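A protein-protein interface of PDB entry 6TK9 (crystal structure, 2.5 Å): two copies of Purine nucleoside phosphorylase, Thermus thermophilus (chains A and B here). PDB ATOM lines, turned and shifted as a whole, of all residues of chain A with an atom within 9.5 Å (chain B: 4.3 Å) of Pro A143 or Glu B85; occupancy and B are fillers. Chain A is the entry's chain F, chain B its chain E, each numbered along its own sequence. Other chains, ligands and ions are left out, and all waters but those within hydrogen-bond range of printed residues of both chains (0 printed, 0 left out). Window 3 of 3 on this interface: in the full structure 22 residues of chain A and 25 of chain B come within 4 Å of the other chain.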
ATOM      1  N   GLU A   1       6.977 -18.749  15.352  1.00  0.00           N
ATOM      2  CA  GLU A   1       6.345 -19.036  14.048  1.00  0.00           C
ATOM      3  C   GLU A   1       6.678 -20.488  13.615  1.00  0.00           C
ATOM      4  O   GLU A   1       5.810 -21.092  12.969  1.00  0.00           O
ATOM      5  CB  GLU A   1       6.719 -17.926  13.042  1.00  0.00           C
ATOM      6  CG  GLU A   1       5.569 -17.492  12.113  1.00  0.00           C
ATOM      7  CD  GLU A   1       5.926 -17.089  10.680  1.00  0.00           C
ATOM      8  OE1 GLU A   1       6.868 -16.301  10.524  1.00  0.00           O
ATOM      9  OE2 GLU A   1       5.261 -17.565   9.708  1.00  0.00           O
ATOM     10  N   LEU A   2       7.833 -21.073  13.986  1.00  0.00           N
ATOM     11  CA  LEU A   2       8.321 -22.417  13.513  1.00  0.00           C
ATOM     12  C   LEU A   2       7.173 -23.433  13.483  1.00  0.00           C
ATOM     13  O   LEU A   2       6.615 -23.751  14.555  1.00  0.00           O
ATOM     14  CB  LEU A   2       9.448 -22.941  14.421  1.00  0.00           C
ATOM     15  CG  LEU A   2      10.327 -24.090  13.891  1.00  0.00           C
ATOM     16  CD1 LEU A   2       9.958 -25.440  14.480  1.00  0.00           C
ATOM     17  CD2 LEU A   2      10.320 -24.179  12.374  1.00  0.00           C
ATOM     18  N   GLU A  90      19.267 -24.675  14.370  1.00  0.00           N
ATOM     19  CA  GLU A  90      17.823 -24.691  13.989  1.00  0.00           C
ATOM     20  C   GLU A  90      17.646 -24.247  12.525  1.00  0.00           C
ATOM     21  O   GLU A  90      16.844 -24.896  11.804  1.00  0.00           O
ATOM     22  CB  GLU A  90      17.006 -23.798  14.924  1.00  0.00           C
ATOM     23  CG  GLU A  90      15.497 -23.942  14.760  1.00  0.00           C
ATOM     24  CD  GLU A  90      14.738 -22.626  14.870  1.00  0.00           C
ATOM     25  OE1 GLU A  90      14.981 -21.897  15.851  1.00  0.00           O
ATOM     26  OE2 GLU A  90      13.936 -22.312  13.960  1.00  0.00           O
ATOM     27  N   ARG A  97      13.528 -30.615   7.734  1.00  0.00           N
ATOM     28  CA  ARG A  97      12.197 -30.511   8.394  1.00  0.00           C
ATOM     29  C   ARG A  97      11.096 -30.243   7.355  1.00  0.00           C
ATOM     30  O   ARG A  97      10.004 -30.835   7.512  1.00  0.00           O
ATOM     31  CB  ARG A  97      12.204 -29.414   9.464  1.00  0.00           C
ATOM     32  CG  ARG A  97      12.743 -29.873  10.806  1.00  0.00           C
ATOM     33  CD  ARG A  97      13.158 -28.724  11.695  1.00  0.00           C
ATOM     34  NE  ARG A  97      13.194 -29.147  13.089  1.00  0.00           N
ATOM     35  CZ  ARG A  97      13.461 -28.354  14.113  1.00  0.00           C
ATOM     36  NH1 ARG A  97      13.748 -27.081  13.915  1.00  0.00           N
ATOM     37  NH2 ARG A  97      13.452 -28.852  15.334  1.00  0.00           N
ATOM     38  N   ASN A 138      22.762 -27.620  19.404  1.00  0.00           N
ATOM     39  CA  ASN A 138      21.690 -28.630  19.230  1.00  0.00           C
ATOM     40  C   ASN A 138      20.532 -27.958  18.502  1.00  0.00           C
ATOM     41  O   ASN A 138      20.092 -26.889  18.900  1.00  0.00           O
ATOM     42  CB  ASN A 138      21.277 -29.213  20.581  1.00  0.00           C
ATOM     43  CG  ASN A 138      20.494 -30.501  20.453  1.00  0.00           C
ATOM     44  OD1 ASN A 138      19.346 -30.503  19.996  1.00  0.00           O
ATOM     45  ND2 ASN A 138      21.100 -31.594  20.891  1.00  0.00           N
ATOM     46  N   PRO A 139      20.017 -28.544  17.406  1.00  0.00           N
ATOM     47  CA  PRO A 139      18.911 -27.933  16.669  1.00  0.00           C
ATOM     48  C   PRO A 139      17.600 -27.774  17.450  1.00  0.00           C
ATOM     49  O   PRO A 139      16.779 -27.014  17.012  1.00  0.00           O
ATOM     50  CB  PRO A 139      18.652 -28.887  15.493  1.00  0.00           C
ATOM     51  CG  PRO A 139      19.339 -30.184  15.883  1.00  0.00           C
ATOM     52  CD  PRO A 139      20.479 -29.802  16.805  1.00  0.00           C
ATOM     53  N   LEU A 140      17.405 -28.523  18.536  1.00  0.00           N
ATOM     54  CA  LEU A 140      16.117 -28.578  19.283  1.00  0.00           C
ATOM     55  C   LEU A 140      16.156 -27.608  20.466  1.00  0.00           C
ATOM     56  O   LEU A 140      15.175 -27.532  21.188  1.00  0.00           O
ATOM     57  CB  LEU A 140      15.893 -30.009  19.779  1.00  0.00           C
ATOM     58  CG  LEU A 140      15.823 -31.091  18.710  1.00  0.00           C
ATOM     59  CD1 LEU A 140      15.613 -32.455  19.338  1.00  0.00           C
ATOM     60  CD2 LEU A 140      14.703 -30.797  17.733  1.00  0.00           C
ATOM     61  N   ARG A 141      17.280 -26.945  20.703  1.00  0.00           N
ATOM     62  CA  ARG A 141      17.375 -25.893  21.741  1.00  0.00           C
ATOM     63  C   ARG A 141      16.271 -24.860  21.488  1.00  0.00           C
ATOM     64  O   ARG A 141      16.244 -24.274  20.397  1.00  0.00           O
ATOM     65  CB  ARG A 141      18.744 -25.208  21.739  1.00  0.00           C
ATOM     66  CG  ARG A 141      18.857 -24.114  22.791  1.00  0.00           C
ATOM     67  CD  ARG A 141      20.268 -23.974  23.292  1.00  0.00           C
ATOM     68  NE  ARG A 141      20.289 -23.049  24.404  1.00  0.00           N
ATOM     69  CZ  ARG A 141      20.420 -21.734  24.293  1.00  0.00           C
ATOM     70  NH1 ARG A 141      20.566 -21.177  23.102  1.00  0.00           N
ATOM     71  NH2 ARG A 141      20.436 -20.980  25.380  1.00  0.00           N
ATOM     72  N   GLY A 142      15.414 -24.650  22.484  1.00  0.00           N
ATOM     73  CA  GLY A 142      14.352 -23.639  22.487  1.00  0.00           C
ATOM     74  C   GLY A 142      13.014 -24.306  22.749  1.00  0.00           C
ATOM     75  O   GLY A 142      12.964 -25.463  23.167  1.00  0.00           O
ATOM     76  N   PRO A 143      11.891 -23.600  22.490  1.00  0.00           N
ATOM     77  CA  PRO A 143      10.574 -24.181  22.737  1.00  0.00           C
ATOM     78  C   PRO A 143      10.436 -25.439  21.866  1.00  0.00           C
ATOM     79  O   PRO A 143      11.108 -25.560  20.871  1.00  0.00           O
ATOM     80  CB  PRO A 143       9.569 -23.069  22.374  1.00  0.00           C
ATOM     81  CG  PRO A 143      10.366 -22.115  21.474  1.00  0.00           C
ATOM     82  CD  PRO A 143      11.823 -22.248  21.900  1.00  0.00           C
ATOM     83  N   ASN A 144       9.574 -26.351  22.291  1.00  0.00           N
ATOM     84  CA  ASN A 144       9.314 -27.618  21.594  1.00  0.00           C
ATOM     85  C   ASN A 144       7.847 -27.644  21.192  1.00  0.00           C
ATOM     86  O   ASN A 144       6.969 -27.532  22.060  1.00  0.00           O
ATOM     87  CB  ASN A 144       9.658 -28.824  22.461  1.00  0.00           C
ATOM     88  CG  ASN A 144       9.320 -30.130  21.772  1.00  0.00           C
ATOM     89  OD1 ASN A 144      10.011 -30.546  20.835  1.00  0.00           O
ATOM     90  ND2 ASN A 144       8.259 -30.768  22.238  1.00  0.00           N
ATOM     91  N   ASP A 145       7.623 -27.825  19.899  1.00  0.00           N
ATOM     92  CA  ASP A 145       6.284 -28.006  19.308  1.00  0.00           C
ATOM     93  C   ASP A 145       6.080 -29.518  19.180  1.00  0.00           C
ATOM     94  O   ASP A 145       6.775 -30.145  18.337  1.00  0.00           O
ATOM     95  CB  ASP A 145       6.191 -27.178  18.024  1.00  0.00           C
ATOM     96  CG  ASP A 145       4.782 -26.960  17.519  1.00  0.00           C
ATOM     97  OD1 ASP A 145       3.923 -27.848  17.750  1.00  0.00           O
ATOM     98  OD2 ASP A 145       4.570 -25.907  16.889  1.00  0.00           O
ATOM     99  N   GLU A 146       5.182 -30.049  20.021  1.00  0.00           N
ATOM    100  CA  GLU A 146       4.701 -31.458  20.080  1.00  0.00           C
ATOM    101  C   GLU A 146       4.245 -31.964  18.709  1.00  0.00           C
ATOM    102  O   GLU A 146       4.206 -33.187  18.552  1.00  0.00           O
ATOM    103  CB  GLU A 146       3.501 -31.556  21.021  1.00  0.00           C
ATOM    104  CG  GLU A 146       3.821 -31.215  22.463  1.00  0.00           C
ATOM    105  CD  GLU A 146       3.895 -32.431  23.368  1.00  0.00           C
ATOM    106  OE1 GLU A 146       5.024 -32.906  23.626  1.00  0.00           O
ATOM    107  OE2 GLU A 146       2.825 -32.892  23.808  1.00  0.00           O
ATOM    108  N   LEU A 148       5.808 -31.462  15.967  1.00  0.00           N
ATOM    109  CA  LEU A 148       7.052 -31.963  15.341  1.00  0.00           C
ATOM    110  C   LEU A 148       7.455 -33.251  16.069  1.00  0.00           C
ATOM    111  O   LEU A 148       7.625 -34.306  15.429  1.00  0.00           O
ATOM    112  CB  LEU A 148       8.119 -30.870  15.425  1.00  0.00           C
ATOM    113  CG  LEU A 148       8.109 -29.878  14.261  1.00  0.00           C
ATOM    114  CD1 LEU A 148       6.935 -28.925  14.365  1.00  0.00           C
ATOM    115  CD2 LEU A 148       9.418 -29.110  14.175  1.00  0.00           C
ATOM    116  N   GLY A 149       7.526 -33.187  17.388  1.00  0.00           N
ATOM    117  CA  GLY A 149       7.969 -34.341  18.171  1.00  0.00           C
ATOM    118  C   GLY A 149       8.192 -33.950  19.618  1.00  0.00           C
ATOM    119  O   GLY A 149       7.864 -32.840  20.052  1.00  0.00           O
ATOM    120  N   PRO A 150       8.780 -34.881  20.388  1.00  0.00           N
ATOM    121  CA  PRO A 150       8.829 -34.748  21.841  1.00  0.00           C
ATOM    122  C   PRO A 150       9.957 -33.823  22.317  1.00  0.00           C
ATOM    123  O   PRO A 150      10.816 -33.485  21.534  1.00  0.00           O
ATOM    124  CB  PRO A 150       9.040 -36.196  22.273  1.00  0.00           C
ATOM    125  CG  PRO A 150       9.886 -36.785  21.151  1.00  0.00           C
ATOM    126  CD  PRO A 150       9.396 -36.113  19.880  1.00  0.00           C
ATOM    127  N   ARG A 151       9.879 -33.396  23.578  1.00  0.00           N
ATOM    128  CA  ARG A 151      10.878 -32.506  24.213  1.00  0.00           C
ATOM    129  C   ARG A 151      12.263 -33.189  24.225  1.00  0.00           C
ATOM    130  O   ARG A 151      13.245 -32.499  23.879  1.00  0.00           O
ATOM    131  CB  ARG A 151      10.413 -32.138  25.628  1.00  0.00           C
ATOM    132  CG  ARG A 151      11.453 -31.403  26.467  1.00  0.00           C
ATOM    133  CD  ARG A 151      11.624 -29.929  26.111  1.00  0.00           C
ATOM    134  NE  ARG A 151      12.324 -29.721  24.860  1.00  0.00           N
ATOM    135  CZ  ARG A 151      12.632 -28.533  24.355  1.00  0.00           C
ATOM    136  NH1 ARG A 151      12.285 -27.427  25.000  1.00  0.00           N
ATOM    137  NH2 ARG A 151      13.280 -28.459  23.200  1.00  0.00           N
ATOM    138  N   PHE A 152      12.340 -34.477  24.605  1.00  0.00           N
ATOM    139  CA  PHE A 152      13.612 -35.226  24.808  1.00  0.00           C
ATOM    140  C   PHE A 152      13.690 -36.477  23.917  1.00  0.00           C
ATOM    141  O   PHE A 152      13.660 -37.616  24.399  1.00  0.00           O
ATOM    142  CB  PHE A 152      13.754 -35.606  26.282  1.00  0.00           C
ATOM    143  CG  PHE A 152      13.611 -34.483  27.277  1.00  0.00           C
ATOM    144  CD1 PHE A 152      14.598 -33.529  27.426  1.00  0.00           C
ATOM    145  CD2 PHE A 152      12.517 -34.429  28.128  1.00  0.00           C
ATOM    146  CE1 PHE A 152      14.477 -32.519  28.371  1.00  0.00           C
ATOM    147  CE2 PHE A 152      12.403 -33.434  29.083  1.00  0.00           C
ATOM    148  CZ  PHE A 152      13.382 -32.475  29.203  1.00  0.00           C
ATOM    149  N   HIS A 221      13.907 -36.338  15.896  1.00  0.00           N
ATOM    150  CA  HIS A 221      12.824 -35.550  16.537  1.00  0.00           C
ATOM    151  C   HIS A 221      11.492 -35.843  15.822  1.00  0.00           C
ATOM    152  O   HIS A 221      10.487 -36.079  16.512  1.00  0.00           O
ATOM    153  CB  HIS A 221      13.197 -34.067  16.557  1.00  0.00           C
ATOM    154  CG  HIS A 221      12.281 -33.220  17.373  1.00  0.00           C
ATOM    155  ND1 HIS A 221      11.570 -32.170  16.825  1.00  0.00           N
ATOM    156  CD2 HIS A 221      11.985 -33.235  18.691  1.00  0.00           C
ATOM    157  CE1 HIS A 221      10.875 -31.574  17.773  1.00  0.00           C
ATOM    158  NE2 HIS A 221      11.109 -32.214  18.925  1.00  0.00           N
ATOM    159  N   VAL B  54      10.688 -18.704  33.282  1.00  0.00           N
ATOM    160  CA  VAL B  54       9.591 -19.640  33.665  1.00  0.00           C
ATOM    161  C   VAL B  54       9.907 -21.060  33.164  1.00  0.00           C
ATOM    162  O   VAL B  54      10.517 -21.196  32.083  1.00  0.00           O
ATOM    163  CB  VAL B  54       8.242 -19.116  33.149  1.00  0.00           C
ATOM    164  CG1 VAL B  54       7.959 -17.727  33.710  1.00  0.00           C
ATOM    165  CG2 VAL B  54       8.171 -19.125  31.633  1.00  0.00           C
ATOM    166  N   SER B  55       9.521 -22.072  33.949  1.00  0.00           N
ATOM    167  CA  SER B  55       9.720 -23.513  33.655  1.00  0.00           C
ATOM    168  C   SER B  55       8.792 -23.911  32.513  1.00  0.00           C
ATOM    169  O   SER B  55       7.592 -23.685  32.658  1.00  0.00           O
ATOM    170  CB  SER B  55       9.454 -24.347  34.883  1.00  0.00           C
ATOM    171  OG  SER B  55      10.331 -23.989  35.950  1.00  0.00           O
ATOM    172  N   THR B  56       9.325 -24.435  31.408  1.00  0.00           N
ATOM    173  CA  THR B  56       8.519 -25.009  30.295  1.00  0.00           C
ATOM    174  C   THR B  56       8.706 -26.530  30.255  1.00  0.00           C
ATOM    175  O   THR B  56       7.917 -27.204  29.541  1.00  0.00           O
ATOM    176  CB  THR B  56       8.865 -24.351  28.951  1.00  0.00           C
ATOM    177  OG1 THR B  56      10.071 -24.926  28.443  1.00  0.00           O
ATOM    178  CG2 THR B  56       9.004 -22.845  29.049  1.00  0.00           C
ATOM    179  N   ALA B  57       9.716 -27.046  30.975  1.00  0.00           N
ATOM    180  CA  ALA B  57      10.089 -28.478  30.989  1.00  0.00           C
ATOM    181  C   ALA B  57       9.042 -29.251  31.786  1.00  0.00           C
ATOM    182  O   ALA B  57       8.526 -28.764  32.797  1.00  0.00           O
ATOM    183  CB  ALA B  57      11.487 -28.696  31.532  1.00  0.00           C
ATOM    184  N   VAL B  81      14.935 -24.031  35.457  1.00  0.00           N
ATOM    185  CA  VAL B  81      14.989 -23.879  33.977  1.00  0.00           C
ATOM    186  C   VAL B  81      16.320 -24.455  33.467  1.00  0.00           C
ATOM    187  O   VAL B  81      17.249 -24.689  34.262  1.00  0.00           O
ATOM    188  CB  VAL B  81      14.766 -22.415  33.561  1.00  0.00           C
ATOM    189  CG1 VAL B  81      13.382 -21.930  33.965  1.00  0.00           C
ATOM    190  CG2 VAL B  81      15.836 -21.487  34.112  1.00  0.00           C
ATOM    191  N   HIS B  82      16.399 -24.675  32.167  1.00  0.00           N
ATOM    192  CA  HIS B  82      17.467 -25.449  31.505  1.00  0.00           C
ATOM    193  C   HIS B  82      17.927 -24.701  30.254  1.00  0.00           C
ATOM    194  O   HIS B  82      17.087 -24.049  29.576  1.00  0.00           O
ATOM    195  CB  HIS B  82      16.967 -26.854  31.152  1.00  0.00           C
ATOM    196  CG  HIS B  82      16.291 -27.562  32.273  1.00  0.00           C
ATOM    197  ND1 HIS B  82      14.946 -27.374  32.566  1.00  0.00           N
ATOM    198  CD2 HIS B  82      16.752 -28.461  33.164  1.00  0.00           C
ATOM    199  CE1 HIS B  82      14.610 -28.131  33.588  1.00  0.00           C
ATOM    200  NE2 HIS B  82      15.701 -28.808  33.974  1.00  0.00           N
ATOM    201  N   TYR B  83      19.216 -24.812  29.966  1.00  0.00           N
ATOM    202  CA  TYR B  83      19.846 -24.239  28.765  1.00  0.00           C
ATOM    203  C   TYR B  83      19.078 -24.719  27.530  1.00  0.00           C
ATOM    204  O   TYR B  83      18.777 -23.902  26.634  1.00  0.00           O
ATOM    205  CB  TYR B  83      21.322 -24.607  28.780  1.00  0.00           C
ATOM    206  CG  TYR B  83      22.109 -24.072  27.623  1.00  0.00           C
ATOM    207  CD1 TYR B  83      22.663 -22.801  27.655  1.00  0.00           C
ATOM    208  CD2 TYR B  83      22.322 -24.856  26.510  1.00  0.00           C
ATOM    209  CE1 TYR B  83      23.404 -22.312  26.590  1.00  0.00           C
ATOM    210  CE2 TYR B  83      23.060 -24.383  25.440  1.00  0.00           C
ATOM    211  CZ  TYR B  83      23.607 -23.114  25.481  1.00  0.00           C
ATOM    212  OH  TYR B  83      24.329 -22.691  24.408  1.00  0.00           O
ATOM    213  N   TYR B  84      18.676 -25.982  27.528  1.00  0.00           N
ATOM    214  CA  TYR B  84      18.010 -26.618  26.368  1.00  0.00           C
ATOM    215  C   TYR B  84      16.694 -25.908  26.047  1.00  0.00           C
ATOM    216  O   TYR B  84      16.268 -26.041  24.900  1.00  0.00           O
ATOM    217  CB  TYR B  84      17.776 -28.113  26.586  1.00  0.00           C
ATOM    218  CG  TYR B  84      16.869 -28.525  27.721  1.00  0.00           C
ATOM    219  CD1 TYR B  84      15.482 -28.420  27.646  1.00  0.00           C
ATOM    220  CD2 TYR B  84      17.403 -29.145  28.840  1.00  0.00           C
ATOM    221  CE1 TYR B  84      14.662 -28.878  28.672  1.00  0.00           C
ATOM    222  CE2 TYR B  84      16.602 -29.603  29.873  1.00  0.00           C
ATOM    223  CZ  TYR B  84      15.225 -29.468  29.795  1.00  0.00           C
ATOM    224  OH  TYR B  84      14.469 -29.920  30.842  1.00  0.00           O
ATOM    225  N   GLU B  85      16.065 -25.233  27.013  1.00  0.00           N
ATOM    226  CA  GLU B  85      14.753 -24.551  26.817  1.00  0.00           C
ATOM    227  C   GLU B  85      14.902 -23.270  25.982  1.00  0.00           C
ATOM    228  O   GLU B  85      13.868 -22.767  25.542  1.00  0.00           O
ATOM    229  CB  GLU B  85      14.117 -24.157  28.147  1.00  0.00           C
ATOM    230  CG  GLU B  85      13.565 -25.327  28.933  1.00  0.00           C
ATOM    231  CD  GLU B  85      12.812 -24.869  30.160  1.00  0.00           C
ATOM    232  OE1 GLU B  85      11.672 -24.376  30.002  1.00  0.00           O
ATOM    233  OE2 GLU B  85      13.385 -24.949  31.262  1.00  0.00           O
ATOM    234  N   GLY B  86      16.122 -22.760  25.784  1.00  0.00           N
ATOM    235  CA  GLY B  86      16.375 -21.476  25.114  1.00  0.00           C
ATOM    236  C   GLY B  86      16.939 -20.427  26.065  1.00  0.00           C
ATOM    237  O   GLY B  86      17.318 -19.364  25.586  1.00  0.00           O
ATOM    238  N   TYR B  87      16.996 -20.680  27.371  1.00  0.00           N
ATOM    239  CA  TYR B  87      17.591 -19.725  28.337  1.00  0.00           C
ATOM    240  C   TYR B  87      19.109 -19.770  28.182  1.00  0.00           C
ATOM    241  O   TYR B  87      19.636 -20.873  27.984  1.00  0.00           O
ATOM    242  CB  TYR B  87      17.132 -20.038  29.759  1.00  0.00           C
ATOM    243  CG  TYR B  87      15.650 -19.884  29.936  1.00  0.00           C
ATOM    244  CD1 TYR B  87      15.020 -18.666  29.725  1.00  0.00           C
ATOM    245  CD2 TYR B  87      14.870 -20.968  30.293  1.00  0.00           C
ATOM    246  CE1 TYR B  87      13.643 -18.534  29.852  1.00  0.00           C
ATOM    247  CE2 TYR B  87      13.498 -20.852  30.437  1.00  0.00           C
ATOM    248  CZ  TYR B  87      12.879 -19.631  30.219  1.00  0.00           C
ATOM    249  OH  TYR B  87      11.527 -19.548  30.370  1.00  0.00           O
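The guanidinium group (NE) of Arg A141 sits at hydrogen-bond distance from the backbone carbonyl oxygen (O) of Tyr B83 (2.8 Å). The backbone carbonyl oxygen (O) of Tyr B84 is in hydrogen-bond range of the backbone NH (N) of Gly A142 (2.9 Å). NH2 of Arg A141 sits at hydrogen-bond distance from O of Tyr B87.
The backbone carbonyl oxygen (O) of Val B54 sits at hydrogen-bond distance from the side-chain hydroxyl (OH) of Tyr B87, at 2.6 Å. OE1 of Glu B85 sits at hydrogen-bond distance from N of Thr B56. The backbone NH (N) of Ala B57 lies within hydrogen-bond range of the side-chain carboxylate (OE1) of Glu B85 (3.4 Å). A ring nitrogen (ND1) of His B82 is in hydrogen-bond range of the side-chain hydroxyl (OH) of Tyr B84 (3.1 Å). The backbone NH (N) of His B82 sits at hydrogen-bond distance from the side-chain carboxylate (OE2) of Glu B85, at 3.2 Å. O of Gly A142 sits at hydrogen-bond distance from NH1 of Arg A151, at 2.8 Å.
Among the printed residues, pairs that only touch across the chains: Gly A142 with Glu B85 (3.2 Å), Phe A152 with Tyr B84 (3.2 Å), Arg A141 with Tyr B84 (3.4 Å), Arg A141 with Gly B86 (3.5 Å), Pro A143 with Glu B85 (3.7 Å) and Gly A142 with Gly B86 (3.8 Å).
Of chain A, only Gly A142 and Pro A143 come within 4 Å of Glu B85. No residue of chain A comes within 4 Å of Thr B56. No residue of chain A comes within 4 Å of Val B81. Of the printed residues of chain A, Tyr B84 touches Arg A141, Gly A142 and Phe A152. Gly B86 touches two residues of chain A. Of the printed residues of chain B, Phe A152 touches Tyr B84. Of the printed residues of chain A, Tyr B83 touches Arg A141. Of the printed residues of chain A, Tyr B87 touches Arg A141. Asn A144 touches none of the printed residues of chain B. The nearest residue of chain A that does not touch Glu B85 is Arg A151 (4.2 Å).
Printed residues of chain B that touch a printed residue of chain A: Tyr B83, Tyr B84, Glu B85, Gly B86 and Tyr B87. Along chain B the printed residues that touch a printed residue of chain A span positions 83 to 87. Printed residues of chain A that touch a printed residue of chain B: Arg A141, Gly A142, Pro A143 and Phe A152. Hydrophobic or aromatic side chains of chain A that line the printed part of chain B: Phe A152. Among the printed residues, no Asp or Glu carboxylate lies within 4 Å of a Lys or Arg side-chain nitrogen of the other chain.
No position is printed for both chains. Of the 9 pairs that touch across the chains among the printed residues, none has its exchanged pair printed and touching as well.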
